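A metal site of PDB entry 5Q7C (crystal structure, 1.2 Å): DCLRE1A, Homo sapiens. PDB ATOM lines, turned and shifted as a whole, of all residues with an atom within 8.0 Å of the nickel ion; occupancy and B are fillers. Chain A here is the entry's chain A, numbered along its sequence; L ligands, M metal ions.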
ATOM      1  N   ASP A  18     -22.630   0.492  33.262  1.00  0.00           N
ATOM      2  CA  ASP A  18     -22.790   0.281  31.807  1.00  0.00           C
ATOM      3  C   ASP A  18     -22.303   1.544  30.962  1.00  0.00           C
ATOM      4  O   ASP A  18     -22.968   1.979  29.989  1.00  0.00           O
ATOM      5  CB  ASP A  18     -24.160  -0.198  31.429  1.00  0.00           C
ATOM      6  CG  ASP A  18     -24.568  -1.542  32.160  1.00  0.00           C
ATOM      7  OD1 ASP A  18     -23.664  -2.185  32.691  1.00  0.00           O
ATOM      8  OD2 ASP A  18     -25.797  -1.848  32.074  1.00  0.00           O
ATOM      9  N   THR A  34     -23.535  -4.655  34.057  1.00  0.00           N
ATOM     10  CA  THR A  34     -24.699  -5.482  34.489  1.00  0.00           C
ATOM     11  C   THR A  34     -24.751  -6.790  33.704  1.00  0.00           C
ATOM     12  O   THR A  34     -25.176  -7.797  34.287  1.00  0.00           O
ATOM     13  CB  THR A  34     -26.041  -4.737  34.375  1.00  0.00           C
ATOM     14  OG1 THR A  34     -26.282  -4.375  32.991  1.00  0.00           O
ATOM     15  CG2 THR A  34     -26.070  -3.486  35.274  1.00  0.00           C
ATOM     16  N   HIS A  35     -24.368  -6.822  32.434  1.00  0.00           N
ATOM     17  CA  HIS A  35     -24.514  -8.016  31.586  1.00  0.00           C
ATOM     18  C   HIS A  35     -23.748  -7.820  30.295  1.00  0.00           C
ATOM     19  O   HIS A  35     -23.491  -6.672  29.851  1.00  0.00           O
ATOM     20  CB  HIS A  35     -26.016  -8.403  31.368  1.00  0.00           C
ATOM     21  CG  HIS A  35     -26.824  -7.456  30.531  1.00  0.00           C
ATOM     22  ND1 HIS A  35     -27.218  -6.167  30.878  1.00  0.00           N
ATOM     23  CD2 HIS A  35     -27.395  -7.636  29.293  1.00  0.00           C
ATOM     24  CE1 HIS A  35     -27.983  -5.665  29.919  1.00  0.00           C
ATOM     25  NE2 HIS A  35     -28.142  -6.551  28.993  1.00  0.00           N
ATOM     26  N   PHE A  36     -23.505  -8.964  29.667  1.00  0.00           N
ATOM     27  CA  PHE A  36     -22.732  -8.966  28.385  1.00  0.00           C
ATOM     28  C   PHE A  36     -23.592  -8.830  27.130  1.00  0.00           C
ATOM     29  O   PHE A  36     -23.710  -9.816  26.345  1.00  0.00           O
ATOM     30  CB  PHE A  36     -21.889 -10.249  28.332  1.00  0.00           C
ATOM     31  CG  PHE A  36     -20.762 -10.235  27.285  1.00  0.00           C
ATOM     32  CD1 PHE A  36     -19.581  -9.517  27.543  1.00  0.00           C
ATOM     33  CD2 PHE A  36     -20.850 -10.983  26.120  1.00  0.00           C
ATOM     34  CE1 PHE A  36     -18.539  -9.500  26.582  1.00  0.00           C
ATOM     35  CE2 PHE A  36     -19.814 -10.989  25.151  1.00  0.00           C
ATOM     36  CZ  PHE A  36     -18.674 -10.279  25.391  1.00  0.00           C
ATOM     37  N   HIS A  37     -24.223  -7.659  26.922  1.00  0.00           N
ATOM     38  CA  HIS A  37     -24.950  -7.281  25.695  1.00  0.00           C
ATOM     39  C   HIS A  37     -24.201  -6.039  25.162  1.00  0.00           C
ATOM     40  O   HIS A  37     -23.820  -5.126  25.920  1.00  0.00           O
ATOM     41  CB  HIS A  37     -26.407  -6.999  25.854  1.00  0.00           C
ATOM     42  CG  HIS A  37     -27.294  -8.241  25.879  1.00  0.00           C
ATOM     43  ND1 HIS A  37     -28.597  -8.242  26.365  1.00  0.00           N
ATOM     44  CD2 HIS A  37     -27.039  -9.500  25.452  1.00  0.00           C
ATOM     45  CE1 HIS A  37     -29.121  -9.457  26.208  1.00  0.00           C
ATOM     46  NE2 HIS A  37     -28.184 -10.235  25.671  1.00  0.00           N
ATOM     47  N   SER A  38     -24.048  -5.954  23.817  1.00  0.00           N
ATOM     48  CA  SER A  38     -23.164  -4.941  23.170  1.00  0.00           C
ATOM     49  C   SER A  38     -23.549  -3.507  23.453  1.00  0.00           C
ATOM     50  O   SER A  38     -22.618  -2.703  23.647  1.00  0.00           O
ATOM     51  CB  SER A  38     -22.920  -5.268  21.691  1.00  0.00           C
ATOM     52  OG  SER A  38     -24.154  -5.202  21.034  1.00  0.00           O
ATOM     53  N   ASP A  39     -24.814  -3.168  23.581  1.00  0.00           N
ATOM     54  CA  ASP A  39     -25.198  -1.735  23.864  1.00  0.00           C
ATOM     55  C   ASP A  39     -24.685  -1.350  25.259  1.00  0.00           C
ATOM     56  O   ASP A  39     -24.496  -0.118  25.549  1.00  0.00           O
ATOM     57  CB  ASP A  39     -26.685  -1.496  23.791  1.00  0.00           C
ATOM     58  CG  ASP A  39     -27.268  -1.368  22.340  1.00  0.00           C
ATOM     59  OD1 ASP A  39     -26.502  -1.378  21.371  1.00  0.00           O
ATOM     60  OD2 ASP A  39     -28.501  -1.246  22.267  1.00  0.00           O
ATOM     61  N   HIS A  40     -24.489  -2.338  26.181  1.00  0.00           N
ATOM     62  CA  HIS A  40     -24.015  -2.077  27.554  1.00  0.00           C
ATOM     63  C   HIS A  40     -22.553  -2.168  27.746  1.00  0.00           C
ATOM     64  O   HIS A  40     -21.966  -1.346  28.499  1.00  0.00           O
ATOM     65  CB  HIS A  40     -24.756  -3.087  28.499  1.00  0.00           C
ATOM     66  CG  HIS A  40     -26.221  -2.883  28.483  1.00  0.00           C
ATOM     67  ND1 HIS A  40     -26.937  -2.203  29.456  1.00  0.00           N
ATOM     68  CD2 HIS A  40     -27.168  -3.282  27.583  1.00  0.00           C
ATOM     69  CE1 HIS A  40     -28.194  -2.123  29.126  1.00  0.00           C
ATOM     70  NE2 HIS A  40     -28.362  -2.740  27.968  1.00  0.00           N
ATOM     71  N   HIS A  96     -32.611 -12.094  33.114  1.00  0.00           N
ATOM     72  CA  HIS A  96     -32.403 -11.576  31.749  1.00  0.00           C
ATOM     73  C   HIS A  96     -31.626 -12.626  31.004  1.00  0.00           C
ATOM     74  O   HIS A  96     -32.215 -13.711  30.790  1.00  0.00           O
ATOM     75  CB  HIS A  96     -31.768 -10.166  31.794  1.00  0.00           C
ATOM     76  CG  HIS A  96     -31.589  -9.443  30.487  1.00  0.00           C
ATOM     77  ND1 HIS A  96     -32.595  -9.265  29.600  1.00  0.00           N
ATOM     78  CD2 HIS A  96     -30.486  -8.870  29.931  1.00  0.00           C
ATOM     79  CE1 HIS A  96     -32.128  -8.570  28.552  1.00  0.00           C
ATOM     80  NE2 HIS A  96     -30.846  -8.330  28.704  1.00  0.00           N
ATOM     81  N   CYS A  97     -30.409 -12.397  30.551  1.00  0.00           N
ATOM     82  CA  CYS A  97     -29.518 -13.409  29.924  1.00  0.00           C
ATOM     83  C   CYS A  97     -28.593 -13.994  30.952  1.00  0.00           C
ATOM     84  O   CYS A  97     -28.470 -13.492  32.053  1.00  0.00           O
ATOM     85  CB  CYS A  97     -28.821 -12.733  28.751  1.00  0.00           C
ATOM     86  SG  CYS A  97     -27.618 -11.405  29.276  1.00  0.00           S
ATOM     87  N   ALA A 100     -26.528 -11.912  33.899  1.00  0.00           N
ATOM     88  CA  ALA A 100     -27.124 -10.600  34.086  1.00  0.00           C
ATOM     89  C   ALA A 100     -27.512 -10.357  35.534  1.00  0.00           C
ATOM     90  O   ALA A 100     -28.151 -11.225  36.173  1.00  0.00           O
ATOM     91  CB  ALA A 100     -28.299 -10.365  33.160  1.00  0.00           C
ATOM     92  N   GLY A 117     -30.351  -3.000  35.860  1.00  0.00           N
ATOM     93  CA  GLY A 117     -29.788  -3.349  34.534  1.00  0.00           C
ATOM     94  C   GLY A 117     -30.926  -3.626  33.615  1.00  0.00           C
ATOM     95  O   GLY A 117     -31.960  -2.955  33.660  1.00  0.00           O
ATOM     96  N   ASP A 118     -30.751  -4.612  32.725  1.00  0.00           N
ATOM     97  CA  ASP A 118     -31.892  -5.200  31.985  1.00  0.00           C
ATOM     98  C   ASP A 118     -32.473  -6.363  32.794  1.00  0.00           C
ATOM     99  O   ASP A 118     -31.716  -7.186  33.346  1.00  0.00           O
ATOM    100  CB  ASP A 118     -31.496  -5.723  30.613  1.00  0.00           C
ATOM    101  CG  ASP A 118     -31.246  -4.650  29.540  1.00  0.00           C
ATOM    102  OD1 ASP A 118     -31.591  -3.447  29.775  1.00  0.00           O
ATOM    103  OD2 ASP A 118     -30.805  -5.008  28.399  1.00  0.00           O
ATOM    104  N   PHE A 119     -33.800  -6.424  32.888  1.00  0.00           N
ATOM    105  CA  PHE A 119     -34.438  -7.470  33.724  1.00  0.00           C
ATOM    106  C   PHE A 119     -35.804  -7.902  33.186  1.00  0.00           C
ATOM    107  O   PHE A 119     -36.478  -7.131  32.508  1.00  0.00           O
ATOM    108  CB  PHE A 119     -34.508  -7.140  35.269  1.00  0.00           C
ATOM    109  CG  PHE A 119     -35.673  -6.285  35.780  1.00  0.00           C
ATOM    110  CD1 PHE A 119     -36.241  -6.538  37.012  1.00  0.00           C
ATOM    111  CD2 PHE A 119     -36.187  -5.194  35.068  1.00  0.00           C
ATOM    112  CE1 PHE A 119     -37.258  -5.748  37.523  1.00  0.00           C
ATOM    113  CE2 PHE A 119     -37.233  -4.375  35.583  1.00  0.00           C
ATOM    114  CZ  PHE A 119     -37.725  -4.672  36.825  1.00  0.00           C
ATOM    115  N   ASP A 141     -35.274  -0.617  34.075  1.00  0.00           N
ATOM    116  CA  ASP A 141     -35.394  -1.065  32.659  1.00  0.00           C
ATOM    117  C   ASP A 141     -36.855  -0.951  32.246  1.00  0.00           C
ATOM    118  O   ASP A 141     -37.737  -1.770  32.563  1.00  0.00           O
ATOM    119  CB  ASP A 141     -34.956  -2.546  32.510  1.00  0.00           C
ATOM    120  CG  ASP A 141     -35.283  -3.183  31.184  1.00  0.00           C
ATOM    121  OD1 ASP A 141     -35.635  -2.446  30.233  1.00  0.00           O
ATOM    122  OD2 ASP A 141     -35.180  -4.463  31.097  1.00  0.00           O
ATOM    123  N   THR A 143     -37.965  -0.889  28.983  1.00  0.00           N
ATOM    124  CA  THR A 143     -38.100  -1.297  27.582  1.00  0.00           C
ATOM    125  C   THR A 143     -39.519  -1.348  27.097  1.00  0.00           C
ATOM    126  O   THR A 143     -39.882  -0.765  26.053  1.00  0.00           O
ATOM    127  CB  THR A 143     -37.350  -2.645  27.315  1.00  0.00           C
ATOM    128  OG1 THR A 143     -35.938  -2.523  27.564  1.00  0.00           O
ATOM    129  CG2 THR A 143     -37.509  -3.126  25.899  1.00  0.00           C
ATOM    130  N   SER A 183     -26.779 -12.771  20.006  1.00  0.00           N
ATOM    131  CA  SER A 183     -26.263 -12.321  21.310  1.00  0.00           C
ATOM    132  C   SER A 183     -26.457 -13.503  22.266  1.00  0.00           C
ATOM    133  O   SER A 183     -27.197 -14.460  21.917  1.00  0.00           O
ATOM    134  CB  SER A 183     -27.045 -11.089  21.873  1.00  0.00           C
ATOM    135  OG  SER A 183     -28.437 -11.412  22.021  1.00  0.00           O
ATOM    136  N   ILE A 184     -25.933 -13.427  23.456  1.00  0.00           N
ATOM    137  CA  ILE A 184     -26.304 -14.380  24.488  1.00  0.00           C
ATOM    138  C   ILE A 184     -27.743 -14.085  24.984  1.00  0.00           C
ATOM    139  O   ILE A 184     -28.298 -12.955  24.749  1.00  0.00           O
ATOM    140  CB  ILE A 184     -25.359 -14.414  25.719  1.00  0.00           C
ATOM    141  CG1 ILE A 184     -25.346 -13.138  26.504  1.00  0.00           C
ATOM    142  CG2 ILE A 184     -23.945 -14.781  25.275  1.00  0.00           C
ATOM    143  CD1 ILE A 184     -24.681 -13.219  27.830  1.00  0.00           C
ATOM    144  N   GLU A 296     -36.901 -11.618  27.221  1.00  0.00           N
ATOM    145  CA  GLU A 296     -36.051 -11.506  28.428  1.00  0.00           C
ATOM    146  C   GLU A 296     -36.153 -10.096  29.120  1.00  0.00           C
ATOM    147  O   GLU A 296     -35.319  -9.703  29.943  1.00  0.00           O
ATOM    148  CB  GLU A 296     -34.618 -11.952  28.231  1.00  0.00           C
ATOM    149  CG  GLU A 296     -34.564 -13.510  27.962  1.00  0.00           C
ATOM    150  CD  GLU A 296     -33.162 -14.108  27.857  1.00  0.00           C
ATOM    151  OE1 GLU A 296     -32.175 -13.399  27.557  1.00  0.00           O
ATOM    152  OE2 GLU A 296     -33.072 -15.414  28.039  1.00  0.00           O
ATOM    153  N   HIS A 297     -37.220  -9.341  28.730  1.00  0.00           N
ATOM    154  CA  HIS A 297     -37.597  -8.099  29.431  1.00  0.00           C
ATOM    155  C   HIS A 297     -38.990  -8.172  30.004  1.00  0.00           C
ATOM    156  O   HIS A 297     -39.871  -8.889  29.484  1.00  0.00           O
ATOM    157  CB  HIS A 297     -37.543  -6.872  28.500  1.00  0.00           C
ATOM    158  CG  HIS A 297     -36.207  -6.507  27.942  1.00  0.00           C
ATOM    159  ND1 HIS A 297     -35.291  -5.704  28.586  1.00  0.00           N
ATOM    160  CD2 HIS A 297     -35.648  -6.795  26.720  1.00  0.00           C
ATOM    161  CE1 HIS A 297     -34.203  -5.596  27.834  1.00  0.00           C
ATOM    162  NE2 HIS A 297     -34.432  -6.212  26.687  1.00  0.00           N
HETATM  163  C1  LIG L   1     -30.358  -6.002  24.220  1.00  0.00           C
HETATM  164  C2  LIG L   1     -31.646  -6.458  24.955  1.00  0.00           C
HETATM  165  C3  LIG L   1     -29.522  -4.987  25.019  1.00  0.00           C
HETATM  166  O1  LIG L   1     -32.761  -6.473  24.424  1.00  0.00           O
HETATM  167  O2  LIG L   1     -31.467  -6.877  26.085  1.00  0.00           O
HETATM  168  O3  LIG L   1     -29.135  -5.210  26.187  1.00  0.00           O
HETATM  169  O4  LIG L   1     -29.101  -3.936  24.405  1.00  0.00           O
HETATM  170 NI    NI M   1     -29.798  -6.709  27.478  1.00  0.00          NI
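Four residues have an atom within 4 Å of the nickel ion: His 35, His 37, His 96 and Asp 118.
The nearest printed residue that does not touch the nickel ion is His 40 (4.2 Å).
The nickel ion is bound by O3 of the ligand (2.1 Å), O2 of the ligand (2.2 Å), OD2 of Asp 118 (2.2 Å), ND1 of His 37 (2.2 Å), NE2 of His 35 (2.3 Å) and NE2 of His 96 (2.3 Å).
OD2 of Asp 118 sits close to NE2 of His 40 (3.4 Å).
ND1 of His 96 sits at hydrogen-bond distance from O of Glu 296, at 2.8 Å.
A ring nitrogen (NE2) of His 37 is in hydrogen-bond range of the backbone carbonyl oxygen (O) of Ile 184 (2.9 Å).
The side-chain hydroxyl (OG1) of Thr 34 lies within hydrogen-bond range of a ring nitrogen (ND1) of His 35, at 2.9 Å.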
